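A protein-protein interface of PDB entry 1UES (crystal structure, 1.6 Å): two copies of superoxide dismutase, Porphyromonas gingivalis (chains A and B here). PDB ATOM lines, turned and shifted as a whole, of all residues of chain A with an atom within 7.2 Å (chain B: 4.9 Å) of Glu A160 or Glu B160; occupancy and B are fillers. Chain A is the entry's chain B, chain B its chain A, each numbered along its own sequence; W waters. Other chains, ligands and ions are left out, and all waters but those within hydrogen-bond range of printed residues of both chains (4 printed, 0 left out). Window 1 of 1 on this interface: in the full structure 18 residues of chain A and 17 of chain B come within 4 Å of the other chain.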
ATOM      1  N   THR A  23      18.892   1.020  12.584  1.00  0.00           N
ATOM      2  CA  THR A  23      19.519  -0.191  13.083  1.00  0.00           C
ATOM      3  C   THR A  23      20.579  -0.698  12.127  1.00  0.00           C
ATOM      4  O   THR A  23      21.655  -1.103  12.553  1.00  0.00           O
ATOM      5  CB  THR A  23      18.469  -1.291  13.359  1.00  0.00           C
ATOM      6  OG1 THR A  23      17.620  -0.846  14.429  1.00  0.00           O
ATOM      7  CG2 THR A  23      19.152  -2.604  13.775  1.00  0.00           C
ATOM      8  N   HIS A  31      28.676  -1.373  14.872  1.00  0.00           N
ATOM      9  CA  HIS A  31      28.991  -2.619  15.567  1.00  0.00           C
ATOM     10  C   HIS A  31      29.890  -3.532  14.743  1.00  0.00           C
ATOM     11  O   HIS A  31      30.948  -3.936  15.196  1.00  0.00           O
ATOM     12  CB  HIS A  31      27.711  -3.375  15.920  1.00  0.00           C
ATOM     13  CG  HIS A  31      26.925  -2.760  17.039  1.00  0.00           C
ATOM     14  ND1 HIS A  31      27.123  -3.075  18.366  1.00  0.00           N
ATOM     15  CD2 HIS A  31      25.914  -1.862  17.013  1.00  0.00           C
ATOM     16  CE1 HIS A  31      26.270  -2.393  19.111  1.00  0.00           C
ATOM     17  NE2 HIS A  31      25.524  -1.648  18.315  1.00  0.00           N
ATOM     18  N   TYR A  35      33.919  -4.749  15.130  1.00  0.00           N
ATOM     19  CA  TYR A  35      34.363  -6.133  15.215  1.00  0.00           C
ATOM     20  C   TYR A  35      35.475  -6.342  14.183  1.00  0.00           C
ATOM     21  O   TYR A  35      36.486  -6.945  14.485  1.00  0.00           O
ATOM     22  CB  TYR A  35      33.200  -7.086  14.920  1.00  0.00           C
ATOM     23  CG  TYR A  35      32.230  -7.214  16.065  1.00  0.00           C
ATOM     24  CD1 TYR A  35      32.682  -7.450  17.365  1.00  0.00           C
ATOM     25  CD2 TYR A  35      30.861  -7.099  15.855  1.00  0.00           C
ATOM     26  CE1 TYR A  35      31.792  -7.572  18.433  1.00  0.00           C
ATOM     27  CE2 TYR A  35      29.957  -7.220  16.917  1.00  0.00           C
ATOM     28  CZ  TYR A  35      30.431  -7.458  18.197  1.00  0.00           C
ATOM     29  OH  TYR A  35      29.535  -7.607  19.240  1.00  0.00           O
ATOM     30  N   GLY A 120      20.506 -13.653  27.536  1.00  0.00           N
ATOM     31  CA  GLY A 120      21.591 -12.705  27.323  1.00  0.00           C
ATOM     32  C   GLY A 120      21.830 -12.483  25.838  1.00  0.00           C
ATOM     33  O   GLY A 120      20.912 -12.651  25.025  1.00  0.00           O
ATOM     34  N   SER A 121      23.060 -12.126  25.483  1.00  0.00           N
ATOM     35  CA  SER A 121      23.380 -11.911  24.082  1.00  0.00           C
ATOM     36  C   SER A 121      23.773 -13.191  23.394  1.00  0.00           C
ATOM     37  O   SER A 121      24.378 -14.116  23.986  1.00  0.00           O
ATOM     38  CB  SER A 121      24.519 -10.918  23.890  1.00  0.00           C
ATOM     39  OG  SER A 121      24.428  -9.802  24.754  1.00  0.00           O
ATOM     40  N   GLY A 122      23.497 -13.236  22.101  1.00  0.00           N
ATOM     41  CA  GLY A 122      23.861 -14.426  21.366  1.00  0.00           C
ATOM     42  C   GLY A 122      23.177 -14.556  20.031  1.00  0.00           C
ATOM     43  O   GLY A 122      22.612 -13.582  19.484  1.00  0.00           O
ATOM     44  N   ASP A 157      20.171 -12.896  15.115  1.00  0.00           N
ATOM     45  CA  ASP A 157      20.989 -12.212  16.114  1.00  0.00           C
ATOM     46  C   ASP A 157      20.079 -11.795  17.263  1.00  0.00           C
ATOM     47  O   ASP A 157      19.111 -11.050  17.057  1.00  0.00           O
ATOM     48  CB  ASP A 157      21.605 -10.975  15.452  1.00  0.00           C
ATOM     49  CG  ASP A 157      22.675 -10.306  16.290  1.00  0.00           C
ATOM     50  OD1 ASP A 157      23.044 -10.809  17.389  1.00  0.00           O
ATOM     51  OD2 ASP A 157      23.157  -9.251  15.800  1.00  0.00           O
ATOM     52  N   VAL A 158      20.370 -12.270  18.472  1.00  0.00           N
ATOM     53  CA  VAL A 158      19.552 -11.862  19.605  1.00  0.00           C
ATOM     54  C   VAL A 158      20.284 -10.950  20.552  1.00  0.00           C
ATOM     55  O   VAL A 158      19.854 -10.739  21.697  1.00  0.00           O
ATOM     56  CB  VAL A 158      18.857 -13.034  20.351  1.00  0.00           C
ATOM     57  CG1 VAL A 158      17.864 -13.693  19.367  1.00  0.00           C
ATOM     58  CG2 VAL A 158      19.865 -14.028  20.887  1.00  0.00           C
ATOM     59  N   TRP A 159      21.409 -10.413  20.083  1.00  0.00           N
ATOM     60  CA  TRP A 159      22.087  -9.381  20.878  1.00  0.00           C
ATOM     61  C   TRP A 159      21.033  -8.253  20.812  1.00  0.00           C
ATOM     62  O   TRP A 159      20.419  -8.037  19.791  1.00  0.00           O
ATOM     63  CB  TRP A 159      23.366  -8.913  20.188  1.00  0.00           C
ATOM     64  CG  TRP A 159      24.559  -9.760  20.497  1.00  0.00           C
ATOM     65  CD1 TRP A 159      24.744 -11.054  20.156  1.00  0.00           C
ATOM     66  CD2 TRP A 159      25.749  -9.337  21.166  1.00  0.00           C
ATOM     67  NE1 TRP A 159      25.983 -11.489  20.565  1.00  0.00           N
ATOM     68  CE2 TRP A 159      26.625 -10.448  21.191  1.00  0.00           C
ATOM     69  CE3 TRP A 159      26.162  -8.121  21.752  1.00  0.00           C
ATOM     70  CZ2 TRP A 159      27.888 -10.395  21.767  1.00  0.00           C
ATOM     71  CZ3 TRP A 159      27.436  -8.069  22.331  1.00  0.00           C
ATOM     72  CH2 TRP A 159      28.277  -9.194  22.336  1.00  0.00           C
ATOM     73  N   GLU A 160      20.800  -7.539  21.903  1.00  0.00           N
ATOM     74  CA  GLU A 160      19.749  -6.540  21.872  1.00  0.00           C
ATOM     75  C   GLU A 160      19.920  -5.436  20.843  1.00  0.00           C
ATOM     76  O   GLU A 160      18.923  -4.876  20.380  1.00  0.00           O
ATOM     77  CB  GLU A 160      19.563  -5.984  23.292  1.00  0.00           C
ATOM     78  CG  GLU A 160      19.062  -7.066  24.274  1.00  0.00           C
ATOM     79  CD  GLU A 160      18.891  -6.538  25.676  1.00  0.00           C
ATOM     80  OE1 GLU A 160      19.860  -5.938  26.190  1.00  0.00           O
ATOM     81  OE2 GLU A 160      17.793  -6.712  26.250  1.00  0.00           O
ATOM     82  N   HIS A 161      21.159  -5.108  20.486  1.00  0.00           N
ATOM     83  CA  HIS A 161      21.390  -4.049  19.493  1.00  0.00           C
ATOM     84  C   HIS A 161      20.789  -4.377  18.126  1.00  0.00           C
ATOM     85  O   HIS A 161      20.509  -3.477  17.335  1.00  0.00           O
ATOM     86  CB  HIS A 161      22.890  -3.734  19.335  1.00  0.00           C
ATOM     87  CG  HIS A 161      23.730  -4.859  18.819  1.00  0.00           C
ATOM     88  ND1 HIS A 161      24.804  -5.347  19.529  1.00  0.00           N
ATOM     89  CD2 HIS A 161      23.706  -5.552  17.651  1.00  0.00           C
ATOM     90  CE1 HIS A 161      25.409  -6.285  18.831  1.00  0.00           C
ATOM     91  NE2 HIS A 161      24.762  -6.434  17.692  1.00  0.00           N
ATOM     92  N   ALA A 162      20.514  -5.650  17.902  1.00  0.00           N
ATOM     93  CA  ALA A 162      19.933  -6.091  16.632  1.00  0.00           C
ATOM     94  C   ALA A 162      18.463  -5.692  16.470  1.00  0.00           C
ATOM     95  O   ALA A 162      17.929  -5.664  15.360  1.00  0.00           O
ATOM     96  CB  ALA A 162      20.097  -7.640  16.497  1.00  0.00           C
ATOM     97  N   TYR A 163      17.792  -5.388  17.574  1.00  0.00           N
ATOM     98  CA  TYR A 163      16.377  -5.065  17.504  1.00  0.00           C
ATOM     99  C   TYR A 163      15.849  -3.986  18.421  1.00  0.00           C
ATOM    100  O   TYR A 163      14.732  -3.501  18.230  1.00  0.00           O
ATOM    101  CB  TYR A 163      15.567  -6.347  17.770  1.00  0.00           C
ATOM    102  CG  TYR A 163      15.843  -7.029  19.113  1.00  0.00           C
ATOM    103  CD1 TYR A 163      15.204  -6.588  20.308  1.00  0.00           C
ATOM    104  CD2 TYR A 163      16.690  -8.132  19.195  1.00  0.00           C
ATOM    105  CE1 TYR A 163      15.412  -7.256  21.527  1.00  0.00           C
ATOM    106  CE2 TYR A 163      16.906  -8.806  20.414  1.00  0.00           C
ATOM    107  CZ  TYR A 163      16.251  -8.346  21.575  1.00  0.00           C
ATOM    108  OH  TYR A 163      16.427  -8.960  22.780  1.00  0.00           O
ATOM    109  N   TYR A 164      16.643  -3.568  19.395  1.00  0.00           N
ATOM    110  CA  TYR A 164      16.141  -2.634  20.370  1.00  0.00           C
ATOM    111  C   TYR A 164      15.513  -1.326  19.916  1.00  0.00           C
ATOM    112  O   TYR A 164      14.517  -0.906  20.470  1.00  0.00           O
ATOM    113  CB  TYR A 164      17.210  -2.333  21.402  1.00  0.00           C
ATOM    114  CG  TYR A 164      16.571  -2.233  22.738  1.00  0.00           C
ATOM    115  CD1 TYR A 164      16.149  -3.380  23.392  1.00  0.00           C
ATOM    116  CD2 TYR A 164      16.284  -1.004  23.310  1.00  0.00           C
ATOM    117  CE1 TYR A 164      15.426  -3.308  24.603  1.00  0.00           C
ATOM    118  CE2 TYR A 164      15.561  -0.913  24.524  1.00  0.00           C
ATOM    119  CZ  TYR A 164      15.140  -2.088  25.149  1.00  0.00           C
ATOM    120  OH  TYR A 164      14.432  -2.009  26.300  1.00  0.00           O
ATOM    121  N   LEU A 165      16.099  -0.711  18.900  1.00  0.00           N
ATOM    122  CA  LEU A 165      15.593   0.567  18.414  1.00  0.00           C
ATOM    123  C   LEU A 165      14.155   0.503  17.912  1.00  0.00           C
ATOM    124  O   LEU A 165      13.420   1.498  17.976  1.00  0.00           O
ATOM    125  CB  LEU A 165      16.509   1.097  17.314  1.00  0.00           C
ATOM    126  CG  LEU A 165      17.929   1.426  17.807  1.00  0.00           C
ATOM    127  CD1 LEU A 165      18.745   1.932  16.659  1.00  0.00           C
ATOM    128  CD2 LEU A 165      17.866   2.476  18.946  1.00  0.00           C
ATOM    129  N   GLN A 168      12.445  -2.753  21.147  1.00  0.00           N
ATOM    130  CA  GLN A 168      12.730  -2.636  22.577  1.00  0.00           C
ATOM    131  C   GLN A 168      12.766  -4.057  23.157  1.00  0.00           C
ATOM    132  O   GLN A 168      13.454  -4.896  22.620  1.00  0.00           O
ATOM    133  CB  GLN A 168      11.697  -1.766  23.308  1.00  0.00           C
ATOM    134  CG  GLN A 168      11.738  -0.284  22.881  1.00  0.00           C
ATOM    135  CD  GLN A 168      10.957  -0.069  21.613  1.00  0.00           C
ATOM    136  OE1 GLN A 168       9.823  -0.524  21.509  1.00  0.00           O
ATOM    137  NE2 GLN A 168      11.560   0.621  20.637  1.00  0.00           N
ATOM    138  N   ASN A 169      11.988  -4.350  24.199  1.00  0.00           N
ATOM    139  CA  ASN A 169      12.036  -5.685  24.814  1.00  0.00           C
ATOM    140  C   ASN A 169      11.337  -6.817  24.071  1.00  0.00           C
ATOM    141  O   ASN A 169      11.477  -7.992  24.438  1.00  0.00           O
ATOM    142  CB  ASN A 169      11.462  -5.628  26.228  1.00  0.00           C
ATOM    143  CG  ASN A 169       9.973  -5.386  26.224  1.00  0.00           C
ATOM    144  OD1 ASN A 169       9.186  -6.239  26.671  1.00  0.00           O
ATOM    145  ND2 ASN A 169       9.565  -4.233  25.723  1.00  0.00           N
ATOM    146  N   ARG A 171      11.604  -9.142  21.917  1.00  0.00           N
ATOM    147  CA  ARG A 171      12.466 -10.001  21.131  1.00  0.00           C
ATOM    148  C   ARG A 171      11.679 -11.039  20.350  1.00  0.00           C
ATOM    149  O   ARG A 171      11.991 -11.320  19.181  1.00  0.00           O
ATOM    150  CB  ARG A 171      13.476 -10.736  22.036  1.00  0.00           C
ATOM    151  CG  ARG A 171      14.460 -11.569  21.255  1.00  0.00           C
ATOM    152  CD  ARG A 171      15.266 -12.535  22.120  1.00  0.00           C
ATOM    153  NE  ARG A 171      16.381 -11.872  22.791  1.00  0.00           N
ATOM    154  CZ  ARG A 171      17.274 -12.496  23.554  1.00  0.00           C
ATOM    155  NH1 ARG A 171      18.260 -11.811  24.128  1.00  0.00           N
ATOM    156  NH2 ARG A 171      17.174 -13.800  23.753  1.00  0.00           N
ATOM    157  N   HIS B  31      11.160  -4.855  31.022  1.00  0.00           N
ATOM    158  CA  HIS B  31      12.180  -5.861  31.339  1.00  0.00           C
ATOM    159  C   HIS B  31      12.106  -6.369  32.757  1.00  0.00           C
ATOM    160  O   HIS B  31      12.094  -7.594  32.989  1.00  0.00           O
ATOM    161  CB  HIS B  31      13.580  -5.304  31.123  1.00  0.00           C
ATOM    162  CG  HIS B  31      13.930  -5.122  29.687  1.00  0.00           C
ATOM    163  ND1 HIS B  31      14.556  -6.090  28.940  1.00  0.00           N
ATOM    164  CD2 HIS B  31      13.758  -4.060  28.863  1.00  0.00           C
ATOM    165  CE1 HIS B  31      14.762  -5.633  27.719  1.00  0.00           C
ATOM    166  NE2 HIS B  31      14.284  -4.408  27.643  1.00  0.00           N
ATOM    167  N   VAL B 158      25.244  -3.240  31.916  1.00  0.00           N
ATOM    168  CA  VAL B 158      25.776  -3.090  30.572  1.00  0.00           C
ATOM    169  C   VAL B 158      25.064  -3.961  29.569  1.00  0.00           C
ATOM    170  O   VAL B 158      25.556  -4.200  28.463  1.00  0.00           O
ATOM    171  CB  VAL B 158      27.334  -3.194  30.487  1.00  0.00           C
ATOM    172  CG1 VAL B 158      27.950  -2.092  31.384  1.00  0.00           C
ATOM    173  CG2 VAL B 158      27.823  -4.580  30.924  1.00  0.00           C
ATOM    174  N   TRP B 159      23.869  -4.406  29.973  1.00  0.00           N
ATOM    175  CA  TRP B 159      22.993  -5.109  29.035  1.00  0.00           C
ATOM    176  C   TRP B 159      22.664  -3.930  28.101  1.00  0.00           C
ATOM    177  O   TRP B 159      22.460  -2.822  28.558  1.00  0.00           O
ATOM    178  CB  TRP B 159      21.694  -5.565  29.713  1.00  0.00           C
ATOM    179  CG  TRP B 159      21.820  -6.906  30.377  1.00  0.00           C
ATOM    180  CD1 TRP B 159      22.623  -7.220  31.427  1.00  0.00           C
ATOM    181  CD2 TRP B 159      21.114  -8.091  30.029  1.00  0.00           C
ATOM    182  NE1 TRP B 159      22.472  -8.544  31.764  1.00  0.00           N
ATOM    183  CE2 TRP B 159      21.546  -9.111  30.918  1.00  0.00           C
ATOM    184  CE3 TRP B 159      20.152  -8.398  29.047  1.00  0.00           C
ATOM    185  CZ2 TRP B 159      21.046 -10.434  30.856  1.00  0.00           C
ATOM    186  CZ3 TRP B 159      19.644  -9.717  28.984  1.00  0.00           C
ATOM    187  CH2 TRP B 159      20.103 -10.719  29.892  1.00  0.00           C
ATOM    188  N   GLU B 160      22.687  -4.167  26.797  1.00  0.00           N
ATOM    189  CA  GLU B 160      22.416  -3.081  25.862  1.00  0.00           C
ATOM    190  C   GLU B 160      21.092  -2.373  26.051  1.00  0.00           C
ATOM    191  O   GLU B 160      20.990  -1.178  25.772  1.00  0.00           O
ATOM    192  CB  GLU B 160      22.558  -3.611  24.421  1.00  0.00           C
ATOM    193  CG  GLU B 160      23.993  -4.008  24.106  1.00  0.00           C
ATOM    194  CD  GLU B 160      24.163  -4.561  22.710  1.00  0.00           C
ATOM    195  OE1 GLU B 160      23.368  -5.446  22.328  1.00  0.00           O
ATOM    196  OE2 GLU B 160      25.074  -4.096  21.994  1.00  0.00           O
ATOM    197  N   HIS B 161      20.071  -3.069  26.544  1.00  0.00           N
ATOM    198  CA  HIS B 161      18.780  -2.415  26.751  1.00  0.00           C
ATOM    199  C   HIS B 161      18.859  -1.252  27.782  1.00  0.00           C
ATOM    200  O   HIS B 161      18.023  -0.387  27.809  1.00  0.00           O
ATOM    201  CB  HIS B 161      17.697  -3.438  27.172  1.00  0.00           C
ATOM    202  CG  HIS B 161      17.928  -4.091  28.497  1.00  0.00           C
ATOM    203  ND1 HIS B 161      18.008  -5.456  28.636  1.00  0.00           N
ATOM    204  CD2 HIS B 161      18.028  -3.583  29.757  1.00  0.00           C
ATOM    205  CE1 HIS B 161      18.144  -5.773  29.905  1.00  0.00           C
ATOM    206  NE2 HIS B 161      18.163  -4.660  30.611  1.00  0.00           N
ATOM    207  N   ALA B 162      19.906  -1.219  28.591  1.00  0.00           N
ATOM    208  CA  ALA B 162      20.041  -0.177  29.588  1.00  0.00           C
ATOM    209  C   ALA B 162      20.402   1.156  28.967  1.00  0.00           C
ATOM    210  O   ALA B 162      20.180   2.171  29.554  1.00  0.00           O
ATOM    211  CB  ALA B 162      21.110  -0.582  30.603  1.00  0.00           C
ATOM    212  N   TYR B 163      20.914   1.145  27.743  1.00  0.00           N
ATOM    213  CA  TYR B 163      21.382   2.413  27.195  1.00  0.00           C
ATOM    214  C   TYR B 163      21.188   2.562  25.704  1.00  0.00           C
ATOM    215  O   TYR B 163      21.402   3.641  25.171  1.00  0.00           O
ATOM    216  CB  TYR B 163      22.902   2.565  27.499  1.00  0.00           C
ATOM    217  CG  TYR B 163      23.810   1.448  26.978  1.00  0.00           C
ATOM    218  CD1 TYR B 163      24.235   1.426  25.630  1.00  0.00           C
ATOM    219  CD2 TYR B 163      24.217   0.391  27.792  1.00  0.00           C
ATOM    220  CE1 TYR B 163      25.033   0.390  25.123  1.00  0.00           C
ATOM    221  CE2 TYR B 163      25.000  -0.645  27.312  1.00  0.00           C
ATOM    222  CZ  TYR B 163      25.418  -0.646  25.964  1.00  0.00           C
ATOM    223  OH  TYR B 163      26.258  -1.603  25.459  1.00  0.00           O
ATOM    224  N   TYR B 164      20.768   1.517  25.017  1.00  0.00           N
ATOM    225  CA  TYR B 164      20.701   1.618  23.569  1.00  0.00           C
ATOM    226  C   TYR B 164      19.798   2.706  22.994  1.00  0.00           C
ATOM    227  O   TYR B 164      20.115   3.308  21.969  1.00  0.00           O
ATOM    228  CB  TYR B 164      20.326   0.259  22.966  1.00  0.00           C
ATOM    229  CG  TYR B 164      21.051   0.044  21.668  1.00  0.00           C
ATOM    230  CD1 TYR B 164      22.388  -0.316  21.663  1.00  0.00           C
ATOM    231  CD2 TYR B 164      20.431   0.292  20.450  1.00  0.00           C
ATOM    232  CE1 TYR B 164      23.120  -0.425  20.470  1.00  0.00           C
ATOM    233  CE2 TYR B 164      21.148   0.185  19.245  1.00  0.00           C
ATOM    234  CZ  TYR B 164      22.505  -0.170  19.276  1.00  0.00           C
ATOM    235  OH  TYR B 164      23.259  -0.192  18.113  1.00  0.00           O
HETATM  236  O   HOH W   1      22.994  -7.696  23.781  1.00  0.00           O
HETATM  237  O   HOH W   2      15.190  -0.358  28.377  1.00  0.00           O
HETATM  238  O   HOH W   3      22.093  -1.619  15.923  1.00  0.00           O
HETATM  239  O   HOH W   4      22.359  -7.015  26.261  1.00  0.00           O
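CE1 of His A31 touches OE2 of Glu B160, at 3.6 Å.
Gly A120 touches Trp B159 (CA to CH2, 3.6 Å).
Trp A159 touches Glu B160 (CE3 to OE1, 3.9 Å).
Glu A160 touches His B31 (OE2 to CE1, 3.5 Å).
CE3 of Trp B159 touches OE1 of Glu A160, at 3.8 Å.
CE1 of Tyr B164 touches CB of His A161, 3.5 Å away.
CE1 of Tyr A164 touches CB of His B161 (3.4 Å).
Tyr B164 touches Leu A165 (CD2 to CD2, 3.7 Å).
CB of Asn A169 touches NE2 of His B31, 3.4 Å away.
Of the printed residues of chain B, His A31 touches Glu B160 and Tyr B164.
Glu B160 touches just these residues of chain A: His A31, Trp A159, Glu A160 and His A161.
Of the printed residues of chain A, Tyr B164 touches His A31 (2.7 Å), His A161 (3.5 Å) and Leu A165 (3.7 Å).
The nearest residue of chain A that does not touch Glu B160 is Ser A121 (5.1 Å).
The side-chain carboxylate of Glu B160 lies within hydrogen-bond range of the backbone NH of Glu A160.
A ring nitrogen (NE2) of His A31 lies within hydrogen-bond range of the side-chain hydroxyl of Tyr B164, 2.7 Å away.
NE2 of His B31 sits at hydrogen-bond distance from OH of Tyr A164, at 2.8 Å.
A ring nitrogen (ND1) of His A161 lies within hydrogen-bond range of the side-chain carboxylate (OE2) of Glu B160 (2.8 Å).
A ring nitrogen (ND1) of His B161 sits at hydrogen-bond distance from the side-chain carboxylate (OE2) of Glu A160, 2.7 Å away.
Water W1 lies within hydrogen-bond range of the side-chain carboxylate of Glu B160 (2.7 Å), the side-chain hydroxyl of Ser A121 (2.7 Å) and the backbone NH of Glu A160 (2.9 Å).
Water W4 lies within hydrogen-bond range of OE1 of Glu A160 (2.7 Å) and N of Glu B160 (2.9 Å).
Water W2 lies within hydrogen-bond range of the side-chain hydroxyl (OH) of Tyr A164 and the backbone carbonyl oxygen (O) of His B161.
Water W3 lies within hydrogen-bond range of O of His A161, OH of Tyr B164 and O of Thr A23.
NH1 of Arg A171 lies within hydrogen-bond range of O of Gly A120 (2.9 Å).
A ring nitrogen (ND1) of His A161 lies close to a ring nitrogen (ND1) of His A31, 3.4 Å away.
The side-chain amide nitrogen (NE2) of Gln A168 lies close to the backbone carbonyl oxygen (O) of Tyr A164 (3.3 Å).
The side-chain carboxylate (OD1) of Asp A157 sits at hydrogen-bond distance from the backbone NH (N) of Trp A159, at 3.2 Å.
The backbone carbonyl oxygen of Gly A122 lies close to the backbone NH of Trp A159.
The backbone carbonyl oxygen (O) of Leu A165 sits at hydrogen-bond distance from the side-chain amide nitrogen (NE2) of Gln A168, at 3.4 Å.
Printed residues of chain B that touch a printed residue of chain A: His B31, Trp B159, Glu B160, His B161 and Tyr B164.
Hydrophobic or aromatic side chains of chain B within 4 Å of the printed part of chain A: His B31, Trp B159, His B161 and Tyr B164.
Along chain B the printed residues that touch a printed residue of chain A span positions 31 to 164.
Among the printed residues, 14 pairs touch across the chains.
His A31 touches Glu B160, and with the chains exchanged Glu A160 touches His B31.
His A31 touches Tyr B164, and with the chains exchanged Tyr A164 touches His B31.
Glu A160 touches His B161, and with the chains exchanged His A161 touches Glu B160.
His A161 touches Tyr B164, and with the chains exchanged Tyr A164 touches His B161.
Positions printed for both chains: 31, 158, 159, 160, 161, 162, 163 and 164.
Of the 14 pairs that touch across the chains among the printed residues, 11 have their exchanged pair printed and touching as well.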
